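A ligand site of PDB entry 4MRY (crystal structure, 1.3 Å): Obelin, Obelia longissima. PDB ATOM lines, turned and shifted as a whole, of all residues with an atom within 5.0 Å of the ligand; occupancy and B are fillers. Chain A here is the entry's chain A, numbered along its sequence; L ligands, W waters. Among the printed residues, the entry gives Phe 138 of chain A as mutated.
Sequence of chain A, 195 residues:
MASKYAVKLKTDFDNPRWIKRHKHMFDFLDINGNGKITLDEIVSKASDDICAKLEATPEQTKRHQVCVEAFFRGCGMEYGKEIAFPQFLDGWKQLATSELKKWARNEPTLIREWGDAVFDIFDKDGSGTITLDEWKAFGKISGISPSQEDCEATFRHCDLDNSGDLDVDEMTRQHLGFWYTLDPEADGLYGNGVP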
ATOM      1  N   HIS A  22     -11.510   4.183  20.713  1.00  0.00           N
ATOM      2  CA  HIS A  22     -10.385   4.917  21.259  1.00  0.00           C
ATOM      3  C   HIS A  22     -10.789   5.876  22.377  1.00  0.00           C
ATOM      4  O   HIS A  22     -10.013   6.064  23.306  1.00  0.00           O
ATOM      5  CB  HIS A  22      -9.578   5.600  20.155  1.00  0.00           C
ATOM      6  CG  HIS A  22      -8.722   4.641  19.397  1.00  0.00           C
ATOM      7  ND1 HIS A  22      -7.536   4.161  19.919  1.00  0.00           N
ATOM      8  CD2 HIS A  22      -8.900   4.008  18.215  1.00  0.00           C
ATOM      9  CE1 HIS A  22      -7.007   3.315  19.065  1.00  0.00           C
ATOM     10  NE2 HIS A  22      -7.813   3.197  18.027  1.00  0.00           N
ATOM     11  N   MET A  25     -10.905   3.912  25.592  1.00  0.00           N
ATOM     12  CA  MET A  25      -9.558   3.670  26.116  1.00  0.00           C
ATOM     13  C   MET A  25      -8.910   4.930  26.676  1.00  0.00           C
ATOM     14  O   MET A  25      -8.277   4.884  27.742  1.00  0.00           O
ATOM     15  CB  MET A  25      -8.660   3.022  25.068  1.00  0.00           C
ATOM     16  CG  MET A  25      -9.078   1.621  24.690  1.00  0.00           C
ATOM     17  SD  MET A  25      -9.190   0.477  26.088  1.00  0.00           S
ATOM     18  CE  MET A  25      -7.574   0.701  26.843  1.00  0.00           C
ATOM     19  N   PHE A  26      -9.041   6.045  25.966  1.00  0.00           N
ATOM     20  CA  PHE A  26      -8.554   7.338  26.441  1.00  0.00           C
ATOM     21  C   PHE A  26      -9.135   7.637  27.825  1.00  0.00           C
ATOM     22  O   PHE A  26      -8.388   7.980  28.749  1.00  0.00           O
ATOM     23  CB  PHE A  26      -8.949   8.410  25.416  1.00  0.00           C
ATOM     24  CG  PHE A  26      -8.547   9.824  25.800  1.00  0.00           C
ATOM     25  CD1 PHE A  26      -9.366  10.622  26.586  1.00  0.00           C
ATOM     26  CD2 PHE A  26      -7.385  10.381  25.295  1.00  0.00           C
ATOM     27  CE1 PHE A  26      -9.000  11.911  26.903  1.00  0.00           C
ATOM     28  CE2 PHE A  26      -7.026  11.689  25.597  1.00  0.00           C
ATOM     29  CZ  PHE A  26      -7.828  12.451  26.399  1.00  0.00           C
ATOM     30  N   PHE A  28     -10.397   5.573  30.017  1.00  0.00           N
ATOM     31  CA  PHE A  28      -9.931   4.596  30.983  1.00  0.00           C
ATOM     32  C   PHE A  28      -8.512   4.907  31.466  1.00  0.00           C
ATOM     33  O   PHE A  28      -8.224   4.846  32.650  1.00  0.00           O
ATOM     34  CB  PHE A  28     -10.004   3.174  30.400  1.00  0.00           C
ATOM     35  CG  PHE A  28      -9.382   2.143  31.285  1.00  0.00           C
ATOM     36  CD1 PHE A  28     -10.030   1.733  32.440  1.00  0.00           C
ATOM     37  CD2 PHE A  28      -8.131   1.636  30.994  1.00  0.00           C
ATOM     38  CE1 PHE A  28      -9.451   0.791  33.280  1.00  0.00           C
ATOM     39  CE2 PHE A  28      -7.542   0.677  31.835  1.00  0.00           C
ATOM     40  CZ  PHE A  28      -8.201   0.260  32.975  1.00  0.00           C
ATOM     41  N   LEU A  29      -7.635   5.246  30.530  1.00  0.00           N
ATOM     42  CA  LEU A  29      -6.239   5.539  30.859  1.00  0.00           C
ATOM     43  C   LEU A  29      -6.049   6.881  31.548  1.00  0.00           C
ATOM     44  O   LEU A  29      -5.036   7.111  32.217  1.00  0.00           O
ATOM     45  CB  LEU A  29      -5.383   5.489  29.599  1.00  0.00           C
ATOM     46  CG  LEU A  29      -5.400   4.138  28.876  1.00  0.00           C
ATOM     47  CD1 LEU A  29      -4.697   4.240  27.530  1.00  0.00           C
ATOM     48  CD2 LEU A  29      -4.775   3.039  29.723  1.00  0.00           C
ATOM     49  N   LYS A  45      -1.200   2.787  33.542  1.00  0.00           N
ATOM     50  CA  LYS A  45      -2.371   1.937  33.350  1.00  0.00           C
ATOM     51  C   LYS A  45      -2.208   0.857  32.275  1.00  0.00           C
ATOM     52  O   LYS A  45      -2.719  -0.245  32.431  1.00  0.00           O
ATOM     53  CB  LYS A  45      -3.594   2.792  33.029  1.00  0.00           C
ATOM     54  CG  LYS A  45      -3.934   3.797  34.100  1.00  0.00           C
ATOM     55  CD  LYS A  45      -4.853   3.187  35.134  1.00  0.00           C
ATOM     56  CE  LYS A  45      -6.194   2.867  34.490  1.00  0.00           C
ATOM     57  NZ  LYS A  45      -7.375   3.405  35.226  1.00  0.00           N
ATOM     58  N   ALA A  46      -1.518   1.189  31.186  1.00  0.00           N
ATOM     59  CA  ALA A  46      -1.369   0.260  30.072  1.00  0.00           C
ATOM     60  C   ALA A  46      -0.109  -0.605  30.183  1.00  0.00           C
ATOM     61  O   ALA A  46       0.048  -1.573  29.433  1.00  0.00           O
ATOM     62  CB  ALA A  46      -1.382   1.007  28.749  1.00  0.00           C
ATOM     63  N   ILE A  50      -0.990  -3.609  33.759  1.00  0.00           N
ATOM     64  CA  ILE A  50      -1.167  -4.789  32.922  1.00  0.00           C
ATOM     65  C   ILE A  50      -0.127  -5.871  33.238  1.00  0.00           C
ATOM     66  O   ILE A  50      -0.471  -7.040  33.400  1.00  0.00           O
ATOM     67  CB  ILE A  50      -1.106  -4.407  31.431  1.00  0.00           C
ATOM     68  CG1 ILE A  50      -2.255  -3.466  31.066  1.00  0.00           C
ATOM     69  CG2 ILE A  50      -1.141  -5.658  30.566  1.00  0.00           C
ATOM     70  CD1 ILE A  50      -3.629  -4.072  31.263  1.00  0.00           C
ATOM     71  N   PHE A  72       3.538   4.816  22.142  1.00  0.00           N
ATOM     72  CA  PHE A  72       2.733   6.014  22.381  1.00  0.00           C
ATOM     73  C   PHE A  72       3.460   7.308  22.032  1.00  0.00           C
ATOM     74  O   PHE A  72       2.813   8.286  21.663  1.00  0.00           O
ATOM     75  CB  PHE A  72       2.091   5.994  23.781  1.00  0.00           C
ATOM     76  CG  PHE A  72       0.945   5.029  23.844  1.00  0.00           C
ATOM     77  CD1 PHE A  72      -0.307   5.406  23.381  1.00  0.00           C
ATOM     78  CD2 PHE A  72       1.142   3.724  24.285  1.00  0.00           C
ATOM     79  CE1 PHE A  72      -1.362   4.501  23.387  1.00  0.00           C
ATOM     80  CE2 PHE A  72       0.073   2.812  24.304  1.00  0.00           C
ATOM     81  CZ  PHE A  72      -1.162   3.211  23.858  1.00  0.00           C
ATOM     82  N   PHE A  88      -4.909  13.159  20.384  1.00  0.00           N
ATOM     83  CA  PHE A  88      -4.560  11.772  20.671  1.00  0.00           C
ATOM     84  C   PHE A  88      -5.034  10.886  19.520  1.00  0.00           C
ATOM     85  O   PHE A  88      -4.281  10.039  19.023  1.00  0.00           O
ATOM     86  CB  PHE A  88      -5.249  11.391  21.980  1.00  0.00           C
ATOM     87  CG  PHE A  88      -5.151   9.938  22.381  1.00  0.00           C
ATOM     88  CD1 PHE A  88      -4.069   9.465  23.083  1.00  0.00           C
ATOM     89  CD2 PHE A  88      -6.205   9.071  22.132  1.00  0.00           C
ATOM     90  CE1 PHE A  88      -4.013   8.138  23.512  1.00  0.00           C
ATOM     91  CE2 PHE A  88      -6.164   7.759  22.552  1.00  0.00           C
ATOM     92  CZ  PHE A  88      -5.075   7.289  23.248  1.00  0.00           C
ATOM     93  N   TRP A  92      -3.028   8.500  16.660  1.00  0.00           N
ATOM     94  CA  TRP A  92      -3.355   7.127  16.274  1.00  0.00           C
ATOM     95  C   TRP A  92      -3.560   6.983  14.764  1.00  0.00           C
ATOM     96  O   TRP A  92      -3.068   6.012  14.186  1.00  0.00           O
ATOM     97  CB  TRP A  92      -4.613   6.662  17.020  1.00  0.00           C
ATOM     98  CG  TRP A  92      -4.345   5.999  18.343  1.00  0.00           C
ATOM     99  CD1 TRP A  92      -4.380   6.572  19.587  1.00  0.00           C
ATOM    100  CD2 TRP A  92      -4.037   4.621  18.539  1.00  0.00           C
ATOM    101  NE1 TRP A  92      -4.104   5.627  20.551  1.00  0.00           N
ATOM    102  CE2 TRP A  92      -3.896   4.428  19.935  1.00  0.00           C
ATOM    103  CE3 TRP A  92      -3.887   3.531  17.690  1.00  0.00           C
ATOM    104  CZ2 TRP A  92      -3.602   3.170  20.483  1.00  0.00           C
ATOM    105  CZ3 TRP A  92      -3.603   2.278  18.230  1.00  0.00           C
ATOM    106  CH2 TRP A  92      -3.469   2.115  19.619  1.00  0.00           C
ATOM    107  N   TRP A 114       5.502  -4.430  20.341  1.00  0.00           N
ATOM    108  CA  TRP A 114       4.684  -4.509  21.552  1.00  0.00           C
ATOM    109  C   TRP A 114       4.097  -5.917  21.665  1.00  0.00           C
ATOM    110  O   TRP A 114       4.115  -6.521  22.751  1.00  0.00           O
ATOM    111  CB  TRP A 114       3.586  -3.462  21.476  1.00  0.00           C
ATOM    112  CG  TRP A 114       2.773  -3.251  22.719  1.00  0.00           C
ATOM    113  CD1 TRP A 114       2.925  -3.855  23.944  1.00  0.00           C
ATOM    114  CD2 TRP A 114       1.681  -2.341  22.845  1.00  0.00           C
ATOM    115  NE1 TRP A 114       1.978  -3.365  24.823  1.00  0.00           N
ATOM    116  CE2 TRP A 114       1.203  -2.445  24.170  1.00  0.00           C
ATOM    117  CE3 TRP A 114       1.049  -1.453  21.961  1.00  0.00           C
ATOM    118  CZ2 TRP A 114       0.140  -1.680  24.638  1.00  0.00           C
ATOM    119  CZ3 TRP A 114      -0.005  -0.705  22.429  1.00  0.00           C
ATOM    120  CH2 TRP A 114      -0.449  -0.813  23.758  1.00  0.00           C
ATOM    121  N   GLY A 115       3.554  -6.428  20.562  1.00  0.00           N
ATOM    122  CA  GLY A 115       3.038  -7.790  20.522  1.00  0.00           C
ATOM    123  C   GLY A 115       4.069  -8.805  20.969  1.00  0.00           C
ATOM    124  O   GLY A 115       3.749  -9.734  21.713  1.00  0.00           O
ATOM    125  N   VAL A 118       4.425  -8.748  24.771  1.00  0.00           N
ATOM    126  CA  VAL A 118       3.278  -9.325  25.463  1.00  0.00           C
ATOM    127  C   VAL A 118       3.198 -10.842  25.225  1.00  0.00           C
ATOM    128  O   VAL A 118       2.927 -11.600  26.146  1.00  0.00           O
ATOM    129  CB  VAL A 118       1.970  -8.636  25.025  1.00  0.00           C
ATOM    130  CG1 VAL A 118       0.750  -9.373  25.551  1.00  0.00           C
ATOM    131  CG2 VAL A 118       1.965  -7.192  25.499  1.00  0.00           C
ATOM    132  N   PHE A 122       2.604 -13.960  27.878  1.00  0.00           N
ATOM    133  CA  PHE A 122       1.565 -14.985  27.782  1.00  0.00           C
ATOM    134  C   PHE A 122       2.132 -16.392  27.618  1.00  0.00           C
ATOM    135  O   PHE A 122       1.522 -17.355  28.074  1.00  0.00           O
ATOM    136  CB  PHE A 122       0.657 -14.730  26.574  1.00  0.00           C
ATOM    137  CG  PHE A 122      -0.254 -13.527  26.692  1.00  0.00           C
ATOM    138  CD1 PHE A 122      -0.686 -13.059  27.923  1.00  0.00           C
ATOM    139  CD2 PHE A 122      -0.700 -12.887  25.545  1.00  0.00           C
ATOM    140  CE1 PHE A 122      -1.540 -11.962  27.995  1.00  0.00           C
ATOM    141  CE2 PHE A 122      -1.558 -11.794  25.609  1.00  0.00           C
ATOM    142  CZ  PHE A 122      -1.966 -11.336  26.828  1.00  0.00           C
ATOM    143  N   PHE A 138      -5.110 -13.564  28.618  1.00  0.00           N
ATOM    144  CA  PHE A 138      -5.549 -12.417  27.818  1.00  0.00           C
ATOM    145  C   PHE A 138      -6.793 -11.792  28.435  1.00  0.00           C
ATOM    146  O   PHE A 138      -6.945 -10.573  28.439  1.00  0.00           O
ATOM    147  CB  PHE A 138      -5.828 -12.840  26.367  1.00  0.00           C
ATOM    148  CG  PHE A 138      -6.080 -11.686  25.442  1.00  0.00           C
ATOM    149  CD1 PHE A 138      -5.026 -11.080  24.775  1.00  0.00           C
ATOM    150  CD2 PHE A 138      -7.364 -11.204  25.235  1.00  0.00           C
ATOM    151  CE1 PHE A 138      -5.246 -10.007  23.937  1.00  0.00           C
ATOM    152  CE2 PHE A 138      -7.596 -10.126  24.403  1.00  0.00           C
ATOM    153  CZ  PHE A 138      -6.532  -9.526  23.744  1.00  0.00           C
ATOM    154  N   ILE A 141      -6.575  -8.841  30.871  1.00  0.00           N
ATOM    155  CA  ILE A 141      -6.240  -7.494  30.380  1.00  0.00           C
ATOM    156  C   ILE A 141      -7.373  -6.512  30.618  1.00  0.00           C
ATOM    157  O   ILE A 141      -7.179  -5.458  31.218  1.00  0.00           O
ATOM    158  CB  ILE A 141      -5.891  -7.491  28.877  1.00  0.00           C
ATOM    159  CG1 ILE A 141      -4.654  -8.347  28.622  1.00  0.00           C
ATOM    160  CG2 ILE A 141      -5.675  -6.074  28.373  1.00  0.00           C
ATOM    161  CD1 ILE A 141      -4.428  -8.629  27.149  1.00  0.00           C
ATOM    162  N   SER A 142      -8.568  -6.848  30.150  1.00  0.00           N
ATOM    163  CA  SER A 142      -9.698  -5.948  30.292  1.00  0.00           C
ATOM    164  C   SER A 142     -10.404  -6.189  31.632  1.00  0.00           C
ATOM    165  O   SER A 142     -10.055  -7.102  32.372  1.00  0.00           O
ATOM    166  CB  SER A 142     -10.682  -6.099  29.144  1.00  0.00           C
ATOM    167  OG  SER A 142     -11.451  -7.275  29.285  1.00  0.00           O
ATOM    168  N   MET A 171      -1.378 -13.262  16.800  1.00  0.00           N
ATOM    169  CA  MET A 171      -1.832 -12.378  17.880  1.00  0.00           C
ATOM    170  C   MET A 171      -1.765 -10.914  17.479  1.00  0.00           C
ATOM    171  O   MET A 171      -2.696 -10.141  17.693  1.00  0.00           O
ATOM    172  CB  MET A 171      -1.038 -12.613  19.167  1.00  0.00           C
ATOM    173  CG  MET A 171      -1.648 -11.903  20.355  1.00  0.00           C
ATOM    174  SD  MET A 171      -0.722 -12.114  21.874  1.00  0.00           S
ATOM    175  CE  MET A 171       0.736 -11.159  21.508  1.00  0.00           C
ATOM    176  N   THR A 172      -0.646 -10.532  16.883  1.00  0.00           N
ATOM    177  CA  THR A 172      -0.456  -9.149  16.460  1.00  0.00           C
ATOM    178  C   THR A 172      -1.466  -8.727  15.416  1.00  0.00           C
ATOM    179  O   THR A 172      -1.950  -7.600  15.423  1.00  0.00           O
ATOM    180  CB  THR A 172       0.978  -8.923  15.921  1.00  0.00           C
ATOM    181  OG1 THR A 172       1.915  -9.201  16.968  1.00  0.00           O
ATOM    182  CG2 THR A 172       1.166  -7.485  15.464  1.00  0.00           C
ATOM    183  N   HIS A 175      -4.560  -7.803  17.265  1.00  0.00           N
ATOM    184  CA  HIS A 175      -4.343  -6.548  17.997  1.00  0.00           C
ATOM    185  C   HIS A 175      -4.386  -5.347  17.030  1.00  0.00           C
ATOM    186  O   HIS A 175      -5.085  -4.365  17.260  1.00  0.00           O
ATOM    187  CB  HIS A 175      -3.003  -6.636  18.754  1.00  0.00           C
ATOM    188  CG  HIS A 175      -2.772  -5.514  19.718  1.00  0.00           C
ATOM    189  ND1 HIS A 175      -1.866  -4.516  19.496  1.00  0.00           N
ATOM    190  CD2 HIS A 175      -3.316  -5.280  20.940  1.00  0.00           C
ATOM    191  CE1 HIS A 175      -1.858  -3.686  20.534  1.00  0.00           C
ATOM    192  NE2 HIS A 175      -2.734  -4.129  21.423  1.00  0.00           N
ATOM    193  N   TRP A 179      -7.218  -2.234  16.840  1.00  0.00           N
ATOM    194  CA  TRP A 179      -6.869  -0.852  17.144  1.00  0.00           C
ATOM    195  C   TRP A 179      -6.578   0.034  15.945  1.00  0.00           C
ATOM    196  O   TRP A 179      -6.918   1.219  15.973  1.00  0.00           O
ATOM    197  CB  TRP A 179      -5.708  -0.802  18.140  1.00  0.00           C
ATOM    198  CG  TRP A 179      -6.007  -1.506  19.423  1.00  0.00           C
ATOM    199  CD1 TRP A 179      -5.376  -2.615  19.892  1.00  0.00           C
ATOM    200  CD2 TRP A 179      -7.029  -1.181  20.379  1.00  0.00           C
ATOM    201  NE1 TRP A 179      -5.915  -2.974  21.107  1.00  0.00           N
ATOM    202  CE2 TRP A 179      -6.931  -2.119  21.420  1.00  0.00           C
ATOM    203  CE3 TRP A 179      -7.988  -0.176  20.469  1.00  0.00           C
ATOM    204  CZ2 TRP A 179      -7.767  -2.097  22.539  1.00  0.00           C
ATOM    205  CZ3 TRP A 179      -8.829  -0.157  21.580  1.00  0.00           C
ATOM    206  CH2 TRP A 179      -8.701  -1.103  22.604  1.00  0.00           C
ATOM    207  N   TYR A 190     -11.687  -8.221  23.011  1.00  0.00           N
ATOM    208  CA  TYR A 190     -11.607  -7.853  24.412  1.00  0.00           C
ATOM    209  C   TYR A 190     -12.933  -8.035  25.153  1.00  0.00           C
ATOM    210  O   TYR A 190     -13.045  -7.668  26.315  1.00  0.00           O
ATOM    211  CB  TYR A 190     -11.170  -6.405  24.545  1.00  0.00           C
ATOM    212  CG  TYR A 190      -9.748  -6.125  24.106  1.00  0.00           C
ATOM    213  CD1 TYR A 190      -8.698  -6.232  25.010  1.00  0.00           C
ATOM    214  CD2 TYR A 190      -9.455  -5.757  22.810  1.00  0.00           C
ATOM    215  CE1 TYR A 190      -7.382  -5.963  24.607  1.00  0.00           C
ATOM    216  CE2 TYR A 190      -8.163  -5.501  22.403  1.00  0.00           C
ATOM    217  CZ  TYR A 190      -7.130  -5.606  23.305  1.00  0.00           C
ATOM    218  OH  TYR A 190      -5.848  -5.333  22.898  1.00  0.00           O
ATOM    219  N   VAL A 194     -15.175  -3.606  26.081  1.00  0.00           N
ATOM    220  CA  VAL A 194     -14.310  -2.755  25.262  1.00  0.00           C
ATOM    221  C   VAL A 194     -14.974  -2.645  23.902  1.00  0.00           C
ATOM    222  O   VAL A 194     -14.932  -3.588  23.116  1.00  0.00           O
ATOM    223  CB  VAL A 194     -12.894  -3.370  25.146  1.00  0.00           C
ATOM    224  CG1 VAL A 194     -12.009  -2.534  24.258  1.00  0.00           C
ATOM    225  CG2 VAL A 194     -12.260  -3.531  26.522  1.00  0.00           C
HETATM  226  O1  LIG L   1      -4.096  -5.349  24.768  1.00  0.00           O
HETATM  227  C1  LIG L   1      -2.979  -5.172  25.213  1.00  0.00           C
HETATM  228  C2  LIG L   1      -2.002  -6.279  25.492  1.00  0.00           C
HETATM  229  C3  LIG L   1      -1.542  -6.713  24.116  1.00  0.00           C
HETATM  230  C4  LIG L   1      -0.612  -5.984  23.380  1.00  0.00           C
HETATM  231  C5  LIG L   1      -0.240  -6.406  22.107  1.00  0.00           C
HETATM  232  C6  LIG L   1      -0.791  -7.566  21.556  1.00  0.00           C
HETATM  233  O2  LIG L   1      -0.431  -8.016  20.302  1.00  0.00           O
HETATM  234  C7  LIG L   1      -1.716  -8.292  22.300  1.00  0.00           C
HETATM  235  C8  LIG L   1      -2.081  -7.866  23.567  1.00  0.00           C
HETATM  236  N1  LIG L   1      -2.571  -3.883  25.528  1.00  0.00           N
HETATM  237  C9  LIG L   1      -3.240  -2.674  25.208  1.00  0.00           C
HETATM  238  C10 LIG L   1      -3.697  -1.718  26.097  1.00  0.00           C
HETATM  239  C11 LIG L   1      -3.720  -1.931  27.570  1.00  0.00           C
HETATM  240  C12 LIG L   1      -5.180  -2.202  27.904  1.00  0.00           C
HETATM  241  C13 LIG L   1      -5.756  -1.804  29.107  1.00  0.00           C
HETATM  242  C14 LIG L   1      -7.090  -2.065  29.379  1.00  0.00           C
HETATM  243  C15 LIG L   1      -7.920  -2.716  28.469  1.00  0.00           C
HETATM  244  C16 LIG L   1      -7.370  -3.107  27.256  1.00  0.00           C
HETATM  245  C17 LIG L   1      -6.019  -2.848  26.986  1.00  0.00           C
HETATM  246  N2  LIG L   1      -4.225  -0.575  25.635  1.00  0.00           N
HETATM  247  C18 LIG L   1      -4.337  -0.340  24.316  1.00  0.00           C
HETATM  248  C19 LIG L   1      -3.869  -1.301  23.435  1.00  0.00           C
HETATM  249  N3  LIG L   1      -3.327  -2.449  23.877  1.00  0.00           N
HETATM  250  C20 LIG L   1      -4.882   0.863  23.854  1.00  0.00           C
HETATM  251  C21 LIG L   1      -4.589   2.078  24.502  1.00  0.00           C
HETATM  252  C22 LIG L   1      -5.104   3.286  24.030  1.00  0.00           C
HETATM  253  C23 LIG L   1      -5.914   3.301  22.904  1.00  0.00           C
HETATM  254  O3  LIG L   1      -6.444   4.489  22.451  1.00  0.00           O
HETATM  255  C24 LIG L   1      -6.221   2.112  22.256  1.00  0.00           C
HETATM  256  C25 LIG L   1      -5.688   0.903  22.716  1.00  0.00           C
HETATM  257  O   HOH W   1       0.410  -6.050  18.716  1.00  0.00           O
HETATM  258  O   HOH W   2      -0.406  -3.678  27.468  1.00  0.00           O
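Residues that only touch the ligand: Phe 88 (3.2 Å), Trp 114 (3.3 Å), Trp 179 (3.4 Å), Gly 115 (3.5 Å), Met 25 (3.5 Å), Ile 141 (3.5 Å), Val 118 (3.5 Å), Met 171 (3.6 Å), Leu 29 (3.7 Å), Phe 72 (3.7 Å), Phe 28 (3.7 Å), Ile 50 (3.8 Å), Phe 138 (3.8 Å) and Ala 46 (3.9 Å). Within 4 Å of the ligand: His 22, Met 25, Phe 28, Leu 29, Ala 46, Ile 50, Phe 72, Phe 88, Trp 92, Trp 114, Gly 115, Val 118, Phe 138, Ile 141, Met 171, His 175, Trp 179 and Tyr 190. The nearest printed residue that does not touch the ligand is Thr 172 (4.01 Å).
The side-chain hydroxyl (OH) of Tyr 190 lies within hydrogen-bond range of the indole nitrogen (NE1) of Trp 179, at 3.0 Å. The side-chain amino group (NZ) of Lys 45 sits at hydrogen-bond distance from the backbone carbonyl oxygen (O) of Phe 28 (3.1 Å). The side-chain hydroxyl (OG) of Ser 142 sits at hydrogen-bond distance from the backbone carbonyl oxygen (O) of Tyr 190, at 3.4 Å. NE2 of His 175 lies within hydrogen-bond range of NE1 of Trp 179 (3.4 Å). O of Trp 179 sits at hydrogen-bond distance from NE2 of His 22, at 3.0 Å.
An oxygen (O3) of the ligand lies within hydrogen-bond range of the indole nitrogen (NE1) of Trp 92 (3.2 Å). The side-chain hydroxyl (OH) of Tyr 190 lies within hydrogen-bond range of an oxygen (O1) of the ligand (2.6 Å). ND1 of His 22 is in hydrogen-bond range of O3 of the ligand (2.8 Å). A ring nitrogen (NE2) of His 175 is in hydrogen-bond range of a nitrogen (N3) of the ligand (3.0 Å).
Water W1 lies within hydrogen-bond range of O2 of the ligand and ND1 of His 175. Water W2 lies within hydrogen-bond range of a nitrogen (N1) of the ligand and the backbone carbonyl oxygen of Ala 46.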
